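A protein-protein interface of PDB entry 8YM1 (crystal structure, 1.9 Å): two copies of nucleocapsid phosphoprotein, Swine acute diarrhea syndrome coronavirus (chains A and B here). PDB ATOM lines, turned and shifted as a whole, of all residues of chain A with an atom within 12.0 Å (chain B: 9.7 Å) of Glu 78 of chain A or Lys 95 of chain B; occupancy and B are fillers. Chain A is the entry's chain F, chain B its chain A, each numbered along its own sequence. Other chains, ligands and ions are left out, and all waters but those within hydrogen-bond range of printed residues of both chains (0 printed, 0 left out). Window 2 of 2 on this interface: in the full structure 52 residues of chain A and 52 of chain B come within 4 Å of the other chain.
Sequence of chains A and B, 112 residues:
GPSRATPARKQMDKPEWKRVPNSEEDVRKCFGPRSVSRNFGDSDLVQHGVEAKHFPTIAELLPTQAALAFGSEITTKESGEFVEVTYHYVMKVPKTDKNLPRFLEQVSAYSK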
ATOM      1  N   PRO A  15      22.717 -23.395  11.803  1.00  0.00           N
ATOM      2  CA  PRO A  15      22.142 -24.528  12.520  1.00  0.00           C
ATOM      3  C   PRO A  15      21.519 -25.471  11.487  1.00  0.00           C
ATOM      4  O   PRO A  15      21.016 -25.020  10.460  1.00  0.00           O
ATOM      5  CB  PRO A  15      21.104 -23.913  13.493  1.00  0.00           C
ATOM      6  CG  PRO A  15      20.906 -22.475  12.984  1.00  0.00           C
ATOM      7  CD  PRO A  15      22.198 -22.106  12.273  1.00  0.00           C
ATOM      8  N   TRP A  17      18.816 -26.991  11.049  1.00  0.00           N
ATOM      9  CA  TRP A  17      17.436 -26.784  10.605  1.00  0.00           C
ATOM     10  C   TRP A  17      17.309 -25.569   9.661  1.00  0.00           C
ATOM     11  O   TRP A  17      16.271 -25.400   9.032  1.00  0.00           O
ATOM     12  CB  TRP A  17      16.489 -26.656  11.816  1.00  0.00           C
ATOM     13  CG  TRP A  17      16.794 -25.506  12.741  1.00  0.00           C
ATOM     14  CD1 TRP A  17      16.284 -24.243  12.678  1.00  0.00           C
ATOM     15  CD2 TRP A  17      17.618 -25.547  13.927  1.00  0.00           C
ATOM     16  NE1 TRP A  17      16.759 -23.483  13.715  1.00  0.00           N
ATOM     17  CE2 TRP A  17      17.574 -24.258  14.503  1.00  0.00           C
ATOM     18  CE3 TRP A  17      18.388 -26.541  14.553  1.00  0.00           C
ATOM     19  CZ2 TRP A  17      18.274 -23.939  15.667  1.00  0.00           C
ATOM     20  CZ3 TRP A  17      19.076 -26.224  15.705  1.00  0.00           C
ATOM     21  CH2 TRP A  17      19.016 -24.940  16.255  1.00  0.00           C
ATOM     22  N   ILE A  74       3.370 -30.440  17.672  1.00  0.00           N
ATOM     23  CA  ILE A  74       4.726 -30.151  18.107  1.00  0.00           C
ATOM     24  C   ILE A  74       4.875 -30.528  19.580  1.00  0.00           C
ATOM     25  O   ILE A  74       4.085 -30.102  20.422  1.00  0.00           O
ATOM     26  CB  ILE A  74       5.083 -28.676  17.834  1.00  0.00           C
ATOM     27  CG1 ILE A  74       4.916 -28.338  16.328  1.00  0.00           C
ATOM     28  CG2 ILE A  74       6.496 -28.344  18.337  1.00  0.00           C
ATOM     29  CD1 ILE A  74       5.233 -26.899  15.966  1.00  0.00           C
ATOM     30  N   THR A  75       5.901 -31.351  19.864  1.00  0.00           N
ATOM     31  CA  THR A  75       6.213 -31.790  21.216  1.00  0.00           C
ATOM     32  C   THR A  75       7.689 -31.510  21.491  1.00  0.00           C
ATOM     33  O   THR A  75       8.501 -31.468  20.563  1.00  0.00           O
ATOM     34  CB  THR A  75       5.878 -33.276  21.368  1.00  0.00           C
ATOM     35  OG1 THR A  75       6.631 -33.951  20.364  1.00  0.00           O
ATOM     36  CG2 THR A  75       4.400 -33.566  21.178  1.00  0.00           C
ATOM     37  N   THR A  76       8.017 -31.283  22.770  1.00  0.00           N
ATOM     38  CA  THR A  76       9.383 -30.984  23.178  1.00  0.00           C
ATOM     39  C   THR A  76       9.732 -31.805  24.414  1.00  0.00           C
ATOM     40  O   THR A  76       8.849 -32.210  25.170  1.00  0.00           O
ATOM     41  CB  THR A  76       9.537 -29.483  23.449  1.00  0.00           C
ATOM     42  OG1 THR A  76       8.700 -29.192  24.566  1.00  0.00           O
ATOM     43  CG2 THR A  76       9.147 -28.624  22.260  1.00  0.00           C
ATOM     44  N   LYS A  77      11.033 -32.058  24.589  1.00  0.00           N
ATOM     45  CA  LYS A  77      11.544 -32.745  25.763  1.00  0.00           C
ATOM     46  C   LYS A  77      13.016 -32.370  25.928  1.00  0.00           C
ATOM     47  O   LYS A  77      13.715 -32.147  24.936  1.00  0.00           O
ATOM     48  CB  LYS A  77      11.356 -34.266  25.640  1.00  0.00           C
ATOM     49  CG  LYS A  77      12.325 -34.987  24.705  1.00  0.00           C
ATOM     50  CD  LYS A  77      11.963 -36.445  24.448  1.00  0.00           C
ATOM     51  CE  LYS A  77      13.072 -37.199  23.788  1.00  0.00           C
ATOM     52  NZ  LYS A  77      12.658 -38.546  23.385  1.00  0.00           N
ATOM     53  N   GLU A  78      13.458 -32.243  27.183  1.00  0.00           N
ATOM     54  CA  GLU A  78      14.838 -31.892  27.471  1.00  0.00           C
ATOM     55  C   GLU A  78      15.728 -33.101  27.190  1.00  0.00           C
ATOM     56  O   GLU A  78      15.344 -34.237  27.463  1.00  0.00           O
ATOM     57  CB  GLU A  78      14.995 -31.400  28.908  1.00  0.00           C
ATOM     58  CG  GLU A  78      14.184 -30.139  29.202  1.00  0.00           C
ATOM     59  CD  GLU A  78      14.403 -29.546  30.583  1.00  0.00           C
ATOM     60  OE1 GLU A  78      15.215 -30.101  31.358  1.00  0.00           O
ATOM     61  OE2 GLU A  78      13.759 -28.520  30.883  1.00  0.00           O
ATOM     62  N   SER A  79      16.894 -32.836  26.583  1.00  0.00           N
ATOM     63  CA  SER A  79      17.853 -33.874  26.242  1.00  0.00           C
ATOM     64  C   SER A  79      19.270 -33.320  26.384  1.00  0.00           C
ATOM     65  O   SER A  79      19.791 -32.695  25.461  1.00  0.00           O
ATOM     66  CB  SER A  79      17.601 -34.409  24.846  1.00  0.00           C
ATOM     67  OG  SER A  79      18.528 -35.432  24.513  1.00  0.00           O
ATOM     68  N   GLY A  80      19.865 -33.525  27.568  1.00  0.00           N
ATOM     69  CA  GLY A  80      21.193 -33.014  27.865  1.00  0.00           C
ATOM     70  C   GLY A  80      21.177 -31.490  27.967  1.00  0.00           C
ATOM     71  O   GLY A  80      20.379 -30.928  28.715  1.00  0.00           O
ATOM     72  N   GLU A  81      21.998 -30.832  27.130  1.00  0.00           N
ATOM     73  CA  GLU A  81      22.080 -29.376  27.100  1.00  0.00           C
ATOM     74  C   GLU A  81      21.227 -28.831  25.945  1.00  0.00           C
ATOM     75  O   GLU A  81      21.438 -27.701  25.497  1.00  0.00           O
ATOM     76  CB  GLU A  81      23.541 -28.936  26.934  1.00  0.00           C
ATOM     77  CG  GLU A  81      24.476 -29.455  28.029  1.00  0.00           C
ATOM     78  CD  GLU A  81      24.216 -28.914  29.430  1.00  0.00           C
ATOM     79  OE1 GLU A  81      23.325 -28.052  29.598  1.00  0.00           O
ATOM     80  OE2 GLU A  81      24.918 -29.364  30.361  1.00  0.00           O
ATOM     81  N   PHE A  82      20.209 -29.615  25.526  1.00  0.00           N
ATOM     82  CA  PHE A  82      19.363 -29.248  24.399  1.00  0.00           C
ATOM     83  C   PHE A  82      17.896 -29.486  24.735  1.00  0.00           C
ATOM     84  O   PHE A  82      17.571 -30.241  25.652  1.00  0.00           O
ATOM     85  CB  PHE A  82      19.686 -30.085  23.153  1.00  0.00           C
ATOM     86  CG  PHE A  82      21.090 -29.923  22.598  1.00  0.00           C
ATOM     87  CD1 PHE A  82      22.133 -30.736  23.039  1.00  0.00           C
ATOM     88  CD2 PHE A  82      21.347 -29.024  21.564  1.00  0.00           C
ATOM     89  CE1 PHE A  82      23.409 -30.606  22.504  1.00  0.00           C
ATOM     90  CE2 PHE A  82      22.624 -28.900  21.032  1.00  0.00           C
ATOM     91  CZ  PHE A  82      23.651 -29.690  21.502  1.00  0.00           C
ATOM     92  N   VAL A  83      17.023 -28.806  23.983  1.00  0.00           N
ATOM     93  CA  VAL A  83      15.601 -29.087  23.983  1.00  0.00           C
ATOM     94  C   VAL A  83      15.276 -29.690  22.621  1.00  0.00           C
ATOM     95  O   VAL A  83      15.516 -29.060  21.589  1.00  0.00           O
ATOM     96  CB  VAL A  83      14.722 -27.851  24.268  1.00  0.00           C
ATOM     97  CG1 VAL A  83      13.241 -28.127  23.999  1.00  0.00           C
ATOM     98  CG2 VAL A  83      14.923 -27.333  25.689  1.00  0.00           C
ATOM     99  N   GLU A  84      14.845 -30.955  22.630  1.00  0.00           N
ATOM    100  CA  GLU A  84      14.519 -31.675  21.410  1.00  0.00           C
ATOM    101  C   GLU A  84      13.094 -31.323  20.987  1.00  0.00           C
ATOM    102  O   GLU A  84      12.148 -31.616  21.707  1.00  0.00           O
ATOM    103  CB  GLU A  84      14.679 -33.177  21.652  1.00  0.00           C
ATOM    104  CG  GLU A  84      14.343 -34.034  20.435  1.00  0.00           C
ATOM    105  CD  GLU A  84      14.437 -35.526  20.695  1.00  0.00           C
ATOM    106  OE1 GLU A  84      15.548 -36.006  21.003  1.00  0.00           O
ATOM    107  OE2 GLU A  84      13.384 -36.196  20.655  1.00  0.00           O
ATOM    108  N   VAL A  85      12.960 -30.720  19.793  1.00  0.00           N
ATOM    109  CA  VAL A  85      11.662 -30.324  19.258  1.00  0.00           C
ATOM    110  C   VAL A  85      11.287 -31.294  18.137  1.00  0.00           C
ATOM    111  O   VAL A  85      12.055 -31.478  17.195  1.00  0.00           O
ATOM    112  CB  VAL A  85      11.688 -28.864  18.749  1.00  0.00           C
ATOM    113  CG1 VAL A  85      10.313 -28.403  18.271  1.00  0.00           C
ATOM    114  CG2 VAL A  85      12.229 -27.905  19.805  1.00  0.00           C
ATOM    115  N   THR A  86      10.096 -31.911  18.256  1.00  0.00           N
ATOM    116  CA  THR A  86       9.607 -32.857  17.259  1.00  0.00           C
ATOM    117  C   THR A  86       8.379 -32.269  16.565  1.00  0.00           C
ATOM    118  O   THR A  86       7.474 -31.766  17.223  1.00  0.00           O
ATOM    119  CB  THR A  86       9.284 -34.198  17.923  1.00  0.00           C
ATOM    120  OG1 THR A  86      10.530 -34.701  18.398  1.00  0.00           O
ATOM    121  CG2 THR A  86       8.673 -35.201  16.957  1.00  0.00           C
ATOM    122  N   LEU B  61      13.435 -20.918  14.987  1.00  0.00           N
ATOM    123  CA  LEU B  61      13.504 -22.331  15.365  1.00  0.00           C
ATOM    124  C   LEU B  61      12.601 -23.191  14.467  1.00  0.00           C
ATOM    125  O   LEU B  61      12.326 -24.342  14.796  1.00  0.00           O
ATOM    126  CB  LEU B  61      13.140 -22.481  16.842  1.00  0.00           C
ATOM    127  CG  LEU B  61      14.066 -21.769  17.834  1.00  0.00           C
ATOM    128  CD1 LEU B  61      13.668 -22.088  19.255  1.00  0.00           C
ATOM    129  CD2 LEU B  61      15.527 -22.132  17.593  1.00  0.00           C
ATOM    130  N   MET B  91      14.589 -31.756  15.757  1.00  0.00           N
ATOM    131  CA  MET B  91      15.712 -30.826  15.833  1.00  0.00           C
ATOM    132  C   MET B  91      16.062 -30.592  17.301  1.00  0.00           C
ATOM    133  O   MET B  91      15.179 -30.586  18.160  1.00  0.00           O
ATOM    134  CB  MET B  91      15.390 -29.493  15.137  1.00  0.00           C
ATOM    135  CG  MET B  91      14.062 -28.875  15.545  1.00  0.00           C
ATOM    136  SD  MET B  91      13.732 -27.301  14.724  1.00  0.00           S
ATOM    137  CE  MET B  91      14.840 -26.185  15.595  1.00  0.00           C
ATOM    138  N   LYS B  92      17.366 -30.418  17.572  1.00  0.00           N
ATOM    139  CA  LYS B  92      17.866 -30.236  18.927  1.00  0.00           C
ATOM    140  C   LYS B  92      18.360 -28.800  19.081  1.00  0.00           C
ATOM    141  O   LYS B  92      19.348 -28.411  18.464  1.00  0.00           O
ATOM    142  CB  LYS B  92      18.966 -31.266  19.207  1.00  0.00           C
ATOM    143  CG  LYS B  92      18.560 -32.711  18.920  1.00  0.00           C
ATOM    144  CD  LYS B  92      19.599 -33.754  19.308  1.00  0.00           C
ATOM    145  CE  LYS B  92      19.169 -35.139  18.932  1.00  0.00           C
ATOM    146  NZ  LYS B  92      20.143 -36.149  19.351  1.00  0.00           N
ATOM    147  N   VAL B  93      17.634 -28.015  19.892  1.00  0.00           N
ATOM    148  CA  VAL B  93      17.933 -26.607  20.091  1.00  0.00           C
ATOM    149  C   VAL B  93      18.728 -26.453  21.386  1.00  0.00           C
ATOM    150  O   VAL B  93      18.310 -26.960  22.426  1.00  0.00           O
ATOM    151  CB  VAL B  93      16.637 -25.774  20.143  1.00  0.00           C
ATOM    152  CG1 VAL B  93      16.925 -24.282  20.292  1.00  0.00           C
ATOM    153  CG2 VAL B  93      15.751 -26.027  18.928  1.00  0.00           C
ATOM    154  N   PRO B  94      19.901 -25.761  21.364  1.00  0.00           N
ATOM    155  CA  PRO B  94      20.650 -25.498  22.595  1.00  0.00           C
ATOM    156  C   PRO B  94      19.773 -24.757  23.606  1.00  0.00           C
ATOM    157  O   PRO B  94      19.010 -23.865  23.233  1.00  0.00           O
ATOM    158  CB  PRO B  94      21.856 -24.647  22.118  1.00  0.00           C
ATOM    159  CG  PRO B  94      22.027 -25.037  20.652  1.00  0.00           C
ATOM    160  CD  PRO B  94      20.623 -25.331  20.155  1.00  0.00           C
ATOM    161  N   LYS B  95      19.920 -25.113  24.892  1.00  0.00           N
ATOM    162  CA  LYS B  95      19.121 -24.516  25.961  1.00  0.00           C
ATOM    163  C   LYS B  95      19.410 -23.011  26.091  1.00  0.00           C
ATOM    164  O   LYS B  95      18.613 -22.284  26.675  1.00  0.00           O
ATOM    165  CB  LYS B  95      19.371 -25.214  27.304  1.00  0.00           C
ATOM    166  CG  LYS B  95      18.736 -26.579  27.467  1.00  0.00           C
ATOM    167  CD  LYS B  95      18.940 -27.158  28.861  1.00  0.00           C
ATOM    168  CE  LYS B  95      18.156 -28.398  29.105  1.00  0.00           C
ATOM    169  NZ  LYS B  95      18.346 -28.884  30.475  1.00  0.00           N
ATOM    170  N   THR B  96      20.553 -22.558  25.540  1.00  0.00           N
ATOM    171  CA  THR B  96      20.962 -21.157  25.633  1.00  0.00           C
ATOM    172  C   THR B  96      20.300 -20.310  24.530  1.00  0.00           C
ATOM    173  O   THR B  96      20.355 -19.084  24.589  1.00  0.00           O
ATOM    174  CB  THR B  96      22.489 -21.071  25.554  1.00  0.00           C
ATOM    175  OG1 THR B  96      22.862 -21.796  24.386  1.00  0.00           O
ATOM    176  CG2 THR B  96      23.172 -21.676  26.766  1.00  0.00           C
ATOM    177  N   ASP B  97      19.666 -20.966  23.536  1.00  0.00           N
ATOM    178  CA  ASP B  97      19.088 -20.256  22.395  1.00  0.00           C
ATOM    179  C   ASP B  97      18.113 -19.180  22.901  1.00  0.00           C
ATOM    180  O   ASP B  97      17.172 -19.481  23.626  1.00  0.00           O
ATOM    181  CB  ASP B  97      18.450 -21.220  21.406  1.00  0.00           C
ATOM    182  CG  ASP B  97      18.070 -20.614  20.062  1.00  0.00           C
ATOM    183  OD1 ASP B  97      18.646 -21.049  19.044  1.00  0.00           O
ATOM    184  OD2 ASP B  97      17.196 -19.723  20.043  1.00  0.00           O
ATOM    185  N   LYS B  98      18.312 -17.938  22.423  1.00  0.00           N
ATOM    186  CA  LYS B  98      17.539 -16.779  22.872  1.00  0.00           C
ATOM    187  C   LYS B  98      16.095 -16.814  22.346  1.00  0.00           C
ATOM    188  O   LYS B  98      15.246 -16.078  22.845  1.00  0.00           O
ATOM    189  CB  LYS B  98      18.224 -15.483  22.420  1.00  0.00           C
ATOM    190  CG  LYS B  98      19.421 -15.066  23.243  1.00  0.00           C
ATOM    191  CD  LYS B  98      20.179 -13.872  22.672  1.00  0.00           C
ATOM    192  CE  LYS B  98      21.025 -13.161  23.700  1.00  0.00           C
ATOM    193  NZ  LYS B  98      21.862 -14.074  24.487  1.00  0.00           N
ATOM    194  N   ASN B  99      15.829 -17.662  21.340  1.00  0.00           N
ATOM    195  CA  ASN B  99      14.518 -17.714  20.699  1.00  0.00           C
ATOM    196  C   ASN B  99      13.655 -18.833  21.304  1.00  0.00           C
ATOM    197  O   ASN B  99      12.452 -18.885  21.051  1.00  0.00           O
ATOM    198  CB  ASN B  99      14.654 -17.931  19.199  1.00  0.00           C
ATOM    199  CG  ASN B  99      15.570 -16.917  18.555  1.00  0.00           C
ATOM    200  OD1 ASN B  99      15.250 -15.727  18.517  1.00  0.00           O
ATOM    201  ND2 ASN B  99      16.698 -17.369  18.024  1.00  0.00           N
ATOM    202  N   LEU B 100      14.267 -19.677  22.151  1.00  0.00           N
ATOM    203  CA  LEU B 100      13.620 -20.892  22.639  1.00  0.00           C
ATOM    204  C   LEU B 100      12.482 -20.569  23.625  1.00  0.00           C
ATOM    205  O   LEU B 100      11.417 -21.172  23.537  1.00  0.00           O
ATOM    206  CB  LEU B 100      14.677 -21.820  23.246  1.00  0.00           C
ATOM    207  CG  LEU B 100      14.185 -23.179  23.752  1.00  0.00           C
ATOM    208  CD1 LEU B 100      13.512 -23.994  22.653  1.00  0.00           C
ATOM    209  CD2 LEU B 100      15.347 -23.943  24.343  1.00  0.00           C
ATOM    210  N   PRO B 101      12.662 -19.645  24.613  1.00  0.00           N
ATOM    211  CA  PRO B 101      11.585 -19.347  25.572  1.00  0.00           C
ATOM    212  C   PRO B 101      10.242 -18.968  24.937  1.00  0.00           C
ATOM    213  O   PRO B 101       9.209 -19.522  25.306  1.00  0.00           O
ATOM    214  CB  PRO B 101      12.196 -18.204  26.387  1.00  0.00           C
ATOM    215  CG  PRO B 101      13.667 -18.552  26.420  1.00  0.00           C
ATOM    216  CD  PRO B 101      13.947 -19.047  25.012  1.00  0.00           C
ATOM    217  N   LEU B 104       8.691 -22.016  23.099  1.00  0.00           N
ATOM    218  CA  LEU B 104       8.091 -22.994  24.010  1.00  0.00           C
ATOM    219  C   LEU B 104       6.719 -22.512  24.504  1.00  0.00           C
ATOM    220  O   LEU B 104       5.831 -23.327  24.736  1.00  0.00           O
ATOM    221  CB  LEU B 104       9.043 -23.268  25.175  1.00  0.00           C
ATOM    222  CG  LEU B 104      10.341 -24.005  24.822  1.00  0.00           C
ATOM    223  CD1 LEU B 104      11.261 -24.097  26.029  1.00  0.00           C
ATOM    224  CD2 LEU B 104      10.048 -25.394  24.269  1.00  0.00           C
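The backbone NH (N) of Val 85 of chain A is in hydrogen-bond range of the backbone carbonyl oxygen (O) of Met 91 of chain B (2.8 Å). The backbone NH (N) of Val 83 of chain A lies within hydrogen-bond range of the backbone carbonyl oxygen (O) of Val 93 of chain B (2.7 Å). The side-chain carboxylate (OE1) of Glu 78 of chain A lies within salt-bridge range of the side-chain amino group (NZ) of Lys 95 of chain B, 3.5 Å away. NZ of Lys 95 of chain B lies within hydrogen-bond range of O of Gly 80 of chain A, at 3.4 Å. N of Lys 95 of chain B lies within hydrogen-bond range of O of Glu 81 of chain A (3.1 Å).
Among the printed residues, merely in contact across the chains: Trp 17 of chain A with Leu 61 of chain B (3.8 Å), Trp 17 of chain A with Met 91 of chain B (3.3 Å), Trp 17 of chain A with Lys 92 of chain B (3.5 Å), Thr 76 of chain A with Leu 104 of chain B (3.9 Å), Glu 81 of chain A with Pro 94 of chain B (3.7 Å), Phe 82 of chain A with Lys 92 of chain B (3.7 Å), Phe 82 of chain A with Val 93 of chain B (3.2 Å), Phe 82 of chain A with Pro 94 of chain B (3.6 Å), Phe 82 of chain A with Lys 95 of chain B (3.9 Å), Val 83 of chain A with Met 91 of chain B (3.8 Å), Val 83 of chain A with Lys 92 of chain B (3.7 Å), Val 83 of chain A with Leu 100 of chain B (3.7 Å) and Glu 84 of chain A with Met 91 of chain B (3.5 Å).
The side-chain amino group (NZ) of Lys 77 of chain A lies within salt-bridge range of the side-chain carboxylate (OE2) of Glu 84 of chain A (3.7 Å).
No position is printed for both chains. Of the 18 pairs that touch across the chains among the printed residues, none has its exchanged pair printed and touching as well.
Of the printed residues of chain B, Trp 17 of chain A touches Leu 61 (3.8 Å), Met 91 (3.3 Å) and Lys 92 (3.5 Å). Thr 75 of chain A touches none of the printed residues of chain B. Glu 78 of chain A touches one residue of chain B. No residue of chain B comes within 4 Å of Ser 79 of chain A. Gly 80 of chain A touches just one residue of chain B: Lys 95 (3.4 Å). Printed residues of chain B within 4 Å of Phe 82 of chain A: Lys 92, Val 93, Pro 94 and Lys 95. Printed residues of chain B within 4 Å of Val 83 of chain A: Met 91 (3.8 Å), Lys 92 (3.7 Å), Val 93 (2.7 Å) and Leu 100 (3.7 Å). Printed residues of chain A within 4 Å of Lys 92 of chain B: Trp 17 (3.5 Å), Phe 82 (3.7 Å) and Val 83 (3.7 Å). Val 93 of chain B touches just these residues of chain A: Phe 82 and Val 83. Of chain A, only Glu 81 (3.7 Å) and Phe 82 (3.6 Å) come within 4 Å of Pro 94 of chain B. Lys 95 of chain B touches four residues of chain A. No residue of chain A comes within 4 Å of Thr 96 of chain B. Asp 97 of chain B touches none of the printed residues of chain A. Of chain A, only Val 83 comes within 4 Å of Leu 100 of chain B. Pro 101 of chain B touches none of the printed residues of chain A. The nearest residue of chain B that does not touch Glu 78 of chain A is Leu 104 of chain B (7.0 Å). The nearest printed residue of chain B that does not touch Val 85 of chain A is Val 93 of chain B (4.1 Å).
Of the 13 printed residues of chain B, 8 touch a printed residue of chain A. Printed residues of chain B that touch a printed residue of chain A: Leu 61, Met 91, Lys 92, Val 93, Pro 94, Lys 95, Leu 100 and Leu 104. Printed residues of chain A that touch a printed residue of chain B: Trp 17, Thr 76, Glu 78, Gly 80, Glu 81, Phe 82, Val 83, Glu 84 and Val 85. Hydrophobic or aromatic side chains of chain A that line the printed part of chain B: Trp 17, Phe 82, Val 83 and Val 85. Among the printed residues, Asp or Glu carboxylates within 4 Å of a Lys or Arg side-chain nitrogen of the other chain: Glu 78 of chain A with Lys 95 of chain B (3.5 Å).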
